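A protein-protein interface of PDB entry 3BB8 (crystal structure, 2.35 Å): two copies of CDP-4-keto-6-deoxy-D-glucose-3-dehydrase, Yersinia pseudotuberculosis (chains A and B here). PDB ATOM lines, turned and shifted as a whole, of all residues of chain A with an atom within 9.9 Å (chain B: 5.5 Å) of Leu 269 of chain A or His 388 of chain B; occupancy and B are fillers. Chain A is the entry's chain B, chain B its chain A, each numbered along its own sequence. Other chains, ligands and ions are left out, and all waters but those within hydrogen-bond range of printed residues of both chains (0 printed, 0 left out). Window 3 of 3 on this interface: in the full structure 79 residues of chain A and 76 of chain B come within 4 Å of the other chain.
Among the printed residues, pairs that only touch across the chains: Tyr 282 of chain A with Pro 385 of chain B (3.3 Å), Ser 283 of chain A with Tyr 386 of chain B (3.3 Å), Gly 270 of chain A with Arg 383 of chain B (3.3 Å), Leu 269 of chain A with His 388 of chain B (3.3 Å), Leu 272 of chain A with Gln 384 of chain B (3.4 Å), His 284 of chain A with Tyr 386 of chain B (3.4 Å), Thr 281 of chain A with Gln 384 of chain B (3.5 Å), Leu 272 of chain A with Arg 383 of chain B (3.6 Å), Leu 285 of chain A with Tyr 386 of chain B (3.7 Å) and Leu 269 of chain A with Pro 385 of chain B (3.7 Å).
Of the 17 printed residues of chain A, 9 touch a printed residue of chain B. Hydrophobic or aromatic side chains of chain A that line the printed part of chain B: Leu 269, Leu 272, Tyr 282 and Leu 285. Printed residues of chain B that touch a printed residue of chain A: Arg 383, Gln 384, Pro 385, Tyr 386 and His 388. Hydrophobic or aromatic side chains of chain B within 4 Å of the printed part of chain A: Pro 385, Tyr 386 and His 388. Among the printed residues, 13 pairs touch across the chains.
N of Tyr 282 of chain A sits close to NE2 of Gln 384 of chain B (2.7 Å). O of Tyr 282 of chain A is in hydrogen-bond range of N of Tyr 386 of chain B (2.9 Å). The guanidinium group (NH1) of Arg 383 of chain B is in hydrogen-bond range of the side-chain hydroxyl (OG) of Ser 271 of chain A, 2.6 Å away.
The backbone NH of Asp 250 of chain A sits at hydrogen-bond distance from the backbone carbonyl oxygen of Thr 281 of chain A. The side-chain carboxylate (OD2) of Asp 389 of chain B is in hydrogen-bond range of a ring nitrogen (ND1) of His 388 of chain B, at 3.1 Å.
No position is printed for both chains. Of the 13 pairs that touch across the chains among the printed residues, none has its exchanged pair printed and touching as well.
Of chain B, only Pro 385 (3.7 Å) and His 388 (3.3 Å) come within 4 Å of Leu 269 of chain A. His 388 of chain B touches just one residue of chain A: Leu 269 (3.3 Å). No residue of chain A comes within 4 Å of Asp 389 of chain B. Printed residues of chain B within 4 Å of Tyr 282 of chain A: Gln 384 (2.7 Å), Pro 385 (3.3 Å) and Tyr 386 (2.9 Å). Of the printed residues of chain B, Ser 271 of chain A touches Arg 383 (2.6 Å). Of the printed residues of chain B, Leu 272 of chain A touches Arg 383 (3.6 Å) and Gln 384 (3.4 Å). Of the printed residues of chain A, Arg 383 of chain B touches Gly 270, Ser 271 and Leu 272. Of the printed residues of chain B, Ser 283 of chain A touches Tyr 386 (3.3 Å). Phe 387 of chain B touches none of the printed residues of chain A. His 278 of chain A touches none of the printed residues of chain B. The nearest printed residue of chain B that does not touch Leu 272 of chain A is Pro 385 of chain B (4.3 Å).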
ATOM      1  N   SER A  99     -12.280 -29.251 -28.408  1.00  0.00           N
ATOM      2  CA  SER A  99     -13.623 -29.600 -27.954  1.00  0.00           C
ATOM      3  C   SER A  99     -13.618 -30.495 -26.723  1.00  0.00           C
ATOM      4  O   SER A  99     -12.973 -31.543 -26.708  1.00  0.00           O
ATOM      5  CB  SER A  99     -14.397 -30.319 -29.051  1.00  0.00           C
ATOM      6  OG  SER A  99     -15.611 -30.833 -28.528  1.00  0.00           O
ATOM      7  N   PRO A 100     -14.355 -30.097 -25.673  1.00  0.00           N
ATOM      8  CA  PRO A 100     -14.392 -30.923 -24.463  1.00  0.00           C
ATOM      9  C   PRO A 100     -14.988 -32.307 -24.744  1.00  0.00           C
ATOM     10  O   PRO A 100     -14.899 -33.205 -23.909  1.00  0.00           O
ATOM     11  CB  PRO A 100     -15.222 -30.082 -23.491  1.00  0.00           C
ATOM     12  CG  PRO A 100     -16.108 -29.273 -24.404  1.00  0.00           C
ATOM     13  CD  PRO A 100     -15.170 -28.879 -25.515  1.00  0.00           C
ATOM     14  N   LYS A 101     -15.579 -32.474 -25.924  1.00  0.00           N
ATOM     15  CA  LYS A 101     -16.147 -33.762 -26.310  1.00  0.00           C
ATOM     16  C   LYS A 101     -15.045 -34.809 -26.536  1.00  0.00           C
ATOM     17  O   LYS A 101     -15.332 -36.005 -26.636  1.00  0.00           O
ATOM     18  CB  LYS A 101     -16.991 -33.632 -27.581  1.00  0.00           C
ATOM     19  CG  LYS A 101     -18.282 -32.845 -27.401  1.00  0.00           C
ATOM     20  CD  LYS A 101     -19.134 -32.901 -28.667  1.00  0.00           C
ATOM     21  CE  LYS A 101     -20.433 -32.112 -28.518  1.00  0.00           C
ATOM     22  NZ  LYS A 101     -21.223 -32.546 -27.326  1.00  0.00           N
ATOM     23  N   ASP A 250     -24.914 -26.351 -31.482  1.00  0.00           N
ATOM     24  CA  ASP A 250     -24.976 -27.778 -31.205  1.00  0.00           C
ATOM     25  C   ASP A 250     -25.451 -28.698 -32.332  1.00  0.00           C
ATOM     26  O   ASP A 250     -25.998 -28.255 -33.335  1.00  0.00           O
ATOM     27  CB  ASP A 250     -25.844 -27.989 -29.968  1.00  0.00           C
ATOM     28  CG  ASP A 250     -25.646 -29.348 -29.340  1.00  0.00           C
ATOM     29  OD1 ASP A 250     -26.117 -30.351 -29.917  1.00  0.00           O
ATOM     30  OD2 ASP A 250     -25.012 -29.408 -28.268  1.00  0.00           O
ATOM     31  N   GLN A 268     -28.173 -32.670 -20.300  1.00  0.00           N
ATOM     32  CA  GLN A 268     -27.244 -31.831 -21.051  1.00  0.00           C
ATOM     33  C   GLN A 268     -26.668 -30.681 -20.218  1.00  0.00           C
ATOM     34  O   GLN A 268     -27.087 -30.445 -19.080  1.00  0.00           O
ATOM     35  CB  GLN A 268     -27.924 -31.281 -22.313  1.00  0.00           C
ATOM     36  CG  GLN A 268     -29.446 -31.443 -22.351  1.00  0.00           C
ATOM     37  CD  GLN A 268     -30.172 -30.568 -21.337  1.00  0.00           C
ATOM     38  OE1 GLN A 268     -31.403 -30.591 -21.252  1.00  0.00           O
ATOM     39  NE2 GLN A 268     -29.415 -29.790 -20.567  1.00  0.00           N
ATOM     40  N   LEU A 269     -25.700 -29.973 -20.797  1.00  0.00           N
ATOM     41  CA  LEU A 269     -25.043 -28.858 -20.118  1.00  0.00           C
ATOM     42  C   LEU A 269     -25.811 -27.548 -20.203  1.00  0.00           C
ATOM     43  O   LEU A 269     -26.732 -27.403 -21.005  1.00  0.00           O
ATOM     44  CB  LEU A 269     -23.641 -28.652 -20.689  1.00  0.00           C
ATOM     45  CG  LEU A 269     -22.621 -29.745 -20.389  1.00  0.00           C
ATOM     46  CD1 LEU A 269     -21.348 -29.465 -21.158  1.00  0.00           C
ATOM     47  CD2 LEU A 269     -22.350 -29.799 -18.894  1.00  0.00           C
ATOM     48  N   GLY A 270     -25.408 -26.592 -19.372  1.00  0.00           N
ATOM     49  CA  GLY A 270     -26.057 -25.297 -19.355  1.00  0.00           C
ATOM     50  C   GLY A 270     -27.401 -25.341 -18.656  1.00  0.00           C
ATOM     51  O   GLY A 270     -27.894 -26.412 -18.305  1.00  0.00           O
ATOM     52  N   SER A 271     -28.000 -24.174 -18.456  1.00  0.00           N
ATOM     53  CA  SER A 271     -29.288 -24.091 -17.791  1.00  0.00           C
ATOM     54  C   SER A 271     -30.335 -23.368 -18.635  1.00  0.00           C
ATOM     55  O   SER A 271     -31.017 -22.461 -18.154  1.00  0.00           O
ATOM     56  CB  SER A 271     -29.125 -23.386 -16.447  1.00  0.00           C
ATOM     57  OG  SER A 271     -28.529 -22.118 -16.614  1.00  0.00           O
ATOM     58  N   LEU A 272     -30.451 -23.768 -19.898  1.00  0.00           N
ATOM     59  CA  LEU A 272     -31.434 -23.173 -20.794  1.00  0.00           C
ATOM     60  C   LEU A 272     -32.798 -23.784 -20.494  1.00  0.00           C
ATOM     61  O   LEU A 272     -32.890 -24.937 -20.068  1.00  0.00           O
ATOM     62  CB  LEU A 272     -31.078 -23.447 -22.257  1.00  0.00           C
ATOM     63  CG  LEU A 272     -29.909 -22.687 -22.882  1.00  0.00           C
ATOM     64  CD1 LEU A 272     -29.743 -23.133 -24.326  1.00  0.00           C
ATOM     65  CD2 LEU A 272     -30.164 -21.187 -22.803  1.00  0.00           C
ATOM     66  N   PRO A 273     -33.879 -23.023 -20.722  1.00  0.00           N
ATOM     67  CA  PRO A 273     -35.215 -23.559 -20.452  1.00  0.00           C
ATOM     68  C   PRO A 273     -35.581 -24.661 -21.440  1.00  0.00           C
ATOM     69  O   PRO A 273     -35.022 -24.738 -22.534  1.00  0.00           O
ATOM     70  CB  PRO A 273     -36.109 -22.331 -20.594  1.00  0.00           C
ATOM     71  CG  PRO A 273     -35.424 -21.567 -21.693  1.00  0.00           C
ATOM     72  CD  PRO A 273     -33.959 -21.668 -21.298  1.00  0.00           C
ATOM     73  N   TYR A 276     -36.063 -24.662 -25.726  1.00  0.00           N
ATOM     74  CA  TYR A 276     -35.238 -23.645 -26.371  1.00  0.00           C
ATOM     75  C   TYR A 276     -34.768 -24.149 -27.734  1.00  0.00           C
ATOM     76  O   TYR A 276     -34.178 -25.221 -27.838  1.00  0.00           O
ATOM     77  CB  TYR A 276     -34.020 -23.310 -25.510  1.00  0.00           C
ATOM     78  CG  TYR A 276     -33.568 -21.881 -25.662  1.00  0.00           C
ATOM     79  CD1 TYR A 276     -34.200 -20.861 -24.960  1.00  0.00           C
ATOM     80  CD2 TYR A 276     -32.542 -21.538 -26.549  1.00  0.00           C
ATOM     81  CE1 TYR A 276     -33.830 -19.534 -25.134  1.00  0.00           C
ATOM     82  CE2 TYR A 276     -32.167 -20.208 -26.733  1.00  0.00           C
ATOM     83  CZ  TYR A 276     -32.818 -19.214 -26.022  1.00  0.00           C
ATOM     84  OH  TYR A 276     -32.477 -17.895 -26.199  1.00  0.00           O
ATOM     85  N   HIS A 278     -33.125 -25.458 -30.837  1.00  0.00           N
ATOM     86  CA  HIS A 278     -31.808 -26.078 -30.942  1.00  0.00           C
ATOM     87  C   HIS A 278     -30.903 -25.191 -31.791  1.00  0.00           C
ATOM     88  O   HIS A 278     -29.718 -25.048 -31.501  1.00  0.00           O
ATOM     89  CB  HIS A 278     -31.889 -27.477 -31.564  1.00  0.00           C
ATOM     90  CG  HIS A 278     -30.801 -28.403 -31.095  1.00  0.00           C
ATOM     91  ND1 HIS A 278     -30.299 -29.428 -31.873  1.00  0.00           N
ATOM     92  CD2 HIS A 278     -30.140 -28.471 -29.913  1.00  0.00           C
ATOM     93  CE1 HIS A 278     -29.378 -30.087 -31.191  1.00  0.00           C
ATOM     94  NE2 HIS A 278     -29.263 -29.527 -29.999  1.00  0.00           N
ATOM     95  N   THR A 281     -28.904 -23.086 -29.713  1.00  0.00           N
ATOM     96  CA  THR A 281     -28.241 -23.758 -28.600  1.00  0.00           C
ATOM     97  C   THR A 281     -26.784 -23.941 -29.058  1.00  0.00           C
ATOM     98  O   THR A 281     -26.520 -24.555 -30.092  1.00  0.00           O
ATOM     99  CB  THR A 281     -28.882 -25.116 -28.316  1.00  0.00           C
ATOM    100  OG1 THR A 281     -30.274 -24.920 -28.039  1.00  0.00           O
ATOM    101  CG2 THR A 281     -28.212 -25.787 -27.109  1.00  0.00           C
ATOM    102  N   TYR A 282     -25.841 -23.409 -28.292  1.00  0.00           N
ATOM    103  CA  TYR A 282     -24.425 -23.460 -28.674  1.00  0.00           C
ATOM    104  C   TYR A 282     -23.500 -24.317 -27.798  1.00  0.00           C
ATOM    105  O   TYR A 282     -23.305 -24.050 -26.615  1.00  0.00           O
ATOM    106  CB  TYR A 282     -23.906 -22.024 -28.746  1.00  0.00           C
ATOM    107  CG  TYR A 282     -24.762 -21.151 -29.635  1.00  0.00           C
ATOM    108  CD1 TYR A 282     -24.619 -21.179 -31.025  1.00  0.00           C
ATOM    109  CD2 TYR A 282     -25.768 -20.344 -29.090  1.00  0.00           C
ATOM    110  CE1 TYR A 282     -25.463 -20.424 -31.855  1.00  0.00           C
ATOM    111  CE2 TYR A 282     -26.608 -19.593 -29.904  1.00  0.00           C
ATOM    112  CZ  TYR A 282     -26.454 -19.637 -31.283  1.00  0.00           C
ATOM    113  OH  TYR A 282     -27.303 -18.911 -32.084  1.00  0.00           O
ATOM    114  N   SER A 283     -22.910 -25.335 -28.414  1.00  0.00           N
ATOM    115  CA  SER A 283     -22.018 -26.256 -27.729  1.00  0.00           C
ATOM    116  C   SER A 283     -20.530 -25.907 -27.818  1.00  0.00           C
ATOM    117  O   SER A 283     -19.729 -26.456 -27.060  1.00  0.00           O
ATOM    118  CB  SER A 283     -22.232 -27.656 -28.286  1.00  0.00           C
ATOM    119  OG  SER A 283     -22.068 -27.655 -29.694  1.00  0.00           O
ATOM    120  N   HIS A 284     -20.149 -25.016 -28.740  1.00  0.00           N
ATOM    121  CA  HIS A 284     -18.728 -24.639 -28.880  1.00  0.00           C
ATOM    122  C   HIS A 284     -18.485 -23.140 -29.035  1.00  0.00           C
ATOM    123  O   HIS A 284     -19.396 -22.385 -29.357  1.00  0.00           O
ATOM    124  CB  HIS A 284     -18.095 -25.342 -30.087  1.00  0.00           C
ATOM    125  CG  HIS A 284     -18.139 -26.837 -30.017  1.00  0.00           C
ATOM    126  ND1 HIS A 284     -17.432 -27.561 -29.080  1.00  0.00           N
ATOM    127  CD2 HIS A 284     -18.785 -27.745 -30.787  1.00  0.00           C
ATOM    128  CE1 HIS A 284     -17.639 -28.851 -29.279  1.00  0.00           C
ATOM    129  NE2 HIS A 284     -18.453 -28.990 -30.309  1.00  0.00           N
ATOM    130  N   LEU A 285     -17.242 -22.727 -28.797  1.00  0.00           N
ATOM    131  CA  LEU A 285     -16.810 -21.337 -28.940  1.00  0.00           C
ATOM    132  C   LEU A 285     -16.569 -21.223 -30.443  1.00  0.00           C
ATOM    133  O   LEU A 285     -15.437 -21.405 -30.918  1.00  0.00           O
ATOM    134  CB  LEU A 285     -15.501 -21.138 -28.183  1.00  0.00           C
ATOM    135  CG  LEU A 285     -14.940 -19.734 -28.002  1.00  0.00           C
ATOM    136  CD1 LEU A 285     -15.950 -18.877 -27.260  1.00  0.00           C
ATOM    137  CD2 LEU A 285     -13.616 -19.822 -27.210  1.00  0.00           C
ATOM    138  N   ARG B 383     -25.788 -19.221 -19.699  1.00  0.00           N
ATOM    139  CA  ARG B 383     -26.508 -20.479 -19.502  1.00  0.00           C
ATOM    140  C   ARG B 383     -26.401 -21.408 -20.707  1.00  0.00           C
ATOM    141  O   ARG B 383     -27.051 -22.458 -20.758  1.00  0.00           O
ATOM    142  CB  ARG B 383     -27.992 -20.222 -19.206  1.00  0.00           C
ATOM    143  CG  ARG B 383     -28.251 -19.459 -17.924  1.00  0.00           C
ATOM    144  CD  ARG B 383     -29.744 -19.302 -17.676  1.00  0.00           C
ATOM    145  NE  ARG B 383     -29.989 -18.558 -16.448  1.00  0.00           N
ATOM    146  CZ  ARG B 383     -29.894 -19.073 -15.228  1.00  0.00           C
ATOM    147  NH1 ARG B 383     -29.567 -20.348 -15.069  1.00  0.00           N
ATOM    148  NH2 ARG B 383     -30.109 -18.304 -14.165  1.00  0.00           N
ATOM    149  N   GLN B 384     -25.605 -21.020 -21.692  1.00  0.00           N
ATOM    150  CA  GLN B 384     -25.438 -21.853 -22.873  1.00  0.00           C
ATOM    151  C   GLN B 384     -24.418 -22.916 -22.538  1.00  0.00           C
ATOM    152  O   GLN B 384     -23.457 -22.651 -21.824  1.00  0.00           O
ATOM    153  CB  GLN B 384     -24.958 -21.015 -24.062  1.00  0.00           C
ATOM    154  CG  GLN B 384     -26.053 -20.176 -24.698  1.00  0.00           C
ATOM    155  CD  GLN B 384     -26.985 -20.997 -25.557  1.00  0.00           C
ATOM    156  OE1 GLN B 384     -28.112 -20.590 -25.832  1.00  0.00           O
ATOM    157  NE2 GLN B 384     -26.514 -22.146 -26.010  1.00  0.00           N
ATOM    158  N   PRO B 385     -24.608 -24.139 -23.047  1.00  0.00           N
ATOM    159  CA  PRO B 385     -23.662 -25.213 -22.761  1.00  0.00           C
ATOM    160  C   PRO B 385     -22.191 -24.911 -23.007  1.00  0.00           C
ATOM    161  O   PRO B 385     -21.355 -25.358 -22.226  1.00  0.00           O
ATOM    162  CB  PRO B 385     -24.172 -26.385 -23.609  1.00  0.00           C
ATOM    163  CG  PRO B 385     -25.124 -25.792 -24.560  1.00  0.00           C
ATOM    164  CD  PRO B 385     -25.749 -24.644 -23.819  1.00  0.00           C
ATOM    165  N   TYR B 386     -21.850 -24.149 -24.054  1.00  0.00           N
ATOM    166  CA  TYR B 386     -20.421 -23.886 -24.294  1.00  0.00           C
ATOM    167  C   TYR B 386     -19.834 -22.920 -23.295  1.00  0.00           C
ATOM    168  O   TYR B 386     -18.626 -22.734 -23.259  1.00  0.00           O
ATOM    169  CB  TYR B 386     -20.143 -23.379 -25.728  1.00  0.00           C
ATOM    170  CG  TYR B 386     -20.351 -21.888 -25.978  1.00  0.00           C
ATOM    171  CD1 TYR B 386     -21.627 -21.372 -26.262  1.00  0.00           C
ATOM    172  CD2 TYR B 386     -19.269 -21.005 -25.983  1.00  0.00           C
ATOM    173  CE1 TYR B 386     -21.816 -20.011 -26.557  1.00  0.00           C
ATOM    174  CE2 TYR B 386     -19.441 -19.639 -26.278  1.00  0.00           C
ATOM    175  CZ  TYR B 386     -20.718 -19.151 -26.568  1.00  0.00           C
ATOM    176  OH  TYR B 386     -20.890 -17.819 -26.896  1.00  0.00           O
ATOM    177  N   PHE B 387     -20.678 -22.301 -22.475  1.00  0.00           N
ATOM    178  CA  PHE B 387     -20.163 -21.368 -21.470  1.00  0.00           C
ATOM    179  C   PHE B 387     -19.866 -22.063 -20.138  1.00  0.00           C
ATOM    180  O   PHE B 387     -19.489 -21.413 -19.166  1.00  0.00           O
ATOM    181  CB  PHE B 387     -21.157 -20.233 -21.221  1.00  0.00           C
ATOM    182  CG  PHE B 387     -20.689 -18.900 -21.722  1.00  0.00           C
ATOM    183  CD1 PHE B 387     -20.782 -18.575 -23.077  1.00  0.00           C
ATOM    184  CD2 PHE B 387     -20.145 -17.966 -20.840  1.00  0.00           C
ATOM    185  CE1 PHE B 387     -20.338 -17.326 -23.549  1.00  0.00           C
ATOM    186  CE2 PHE B 387     -19.699 -16.721 -21.291  1.00  0.00           C
ATOM    187  CZ  PHE B 387     -19.798 -16.397 -22.655  1.00  0.00           C
ATOM    188  N   HIS B 388     -20.026 -23.382 -20.107  1.00  0.00           N
ATOM    189  CA  HIS B 388     -19.807 -24.156 -18.890  1.00  0.00           C
ATOM    190  C   HIS B 388     -18.500 -23.881 -18.165  1.00  0.00           C
ATOM    191  O   HIS B 388     -18.492 -23.757 -16.943  1.00  0.00           O
ATOM    192  CB  HIS B 388     -19.911 -25.652 -19.195  1.00  0.00           C
ATOM    193  CG  HIS B 388     -19.862 -26.525 -17.977  1.00  0.00           C
ATOM    194  ND1 HIS B 388     -18.709 -26.730 -17.251  1.00  0.00           N
ATOM    195  CD2 HIS B 388     -20.827 -27.247 -17.358  1.00  0.00           C
ATOM    196  CE1 HIS B 388     -18.963 -27.542 -16.239  1.00  0.00           C
ATOM    197  NE2 HIS B 388     -20.242 -27.869 -16.282  1.00  0.00           N
ATOM    198  N   ASP B 389     -17.398 -23.775 -18.904  1.00  0.00           N
ATOM    199  CA  ASP B 389     -16.097 -23.538 -18.286  1.00  0.00           C
ATOM    200  C   ASP B 389     -15.413 -22.222 -18.635  1.00  0.00           C
ATOM    201  O   ASP B 389     -14.297 -21.972 -18.196  1.00  0.00           O
ATOM    202  CB  ASP B 389     -15.156 -24.696 -18.621  1.00  0.00           C
ATOM    203  CG  ASP B 389     -15.521 -25.968 -17.884  1.00  0.00           C
ATOM    204  OD1 ASP B 389     -15.547 -27.042 -18.526  1.00  0.00           O
ATOM    205  OD2 ASP B 389     -15.777 -25.890 -16.660  1.00  0.00           O
ATOM    206  N   VAL B 390     -16.074 -21.383 -19.422  1.00  0.00           N
ATOM    207  CA  VAL B 390     -15.505 -20.095 -19.801  1.00  0.00           C
ATOM    208  C   VAL B 390     -15.288 -19.191 -18.585  1.00  0.00           C
ATOM    209  O   VAL B 390     -16.078 -19.193 -17.647  1.00  0.00           O
ATOM    210  CB  VAL B 390     -16.427 -19.361 -20.804  1.00  0.00           C
ATOM    211  CG1 VAL B 390     -15.923 -17.946 -21.048  1.00  0.00           C
ATOM    212  CG2 VAL B 390     -16.488 -20.137 -22.107  1.00  0.00           C
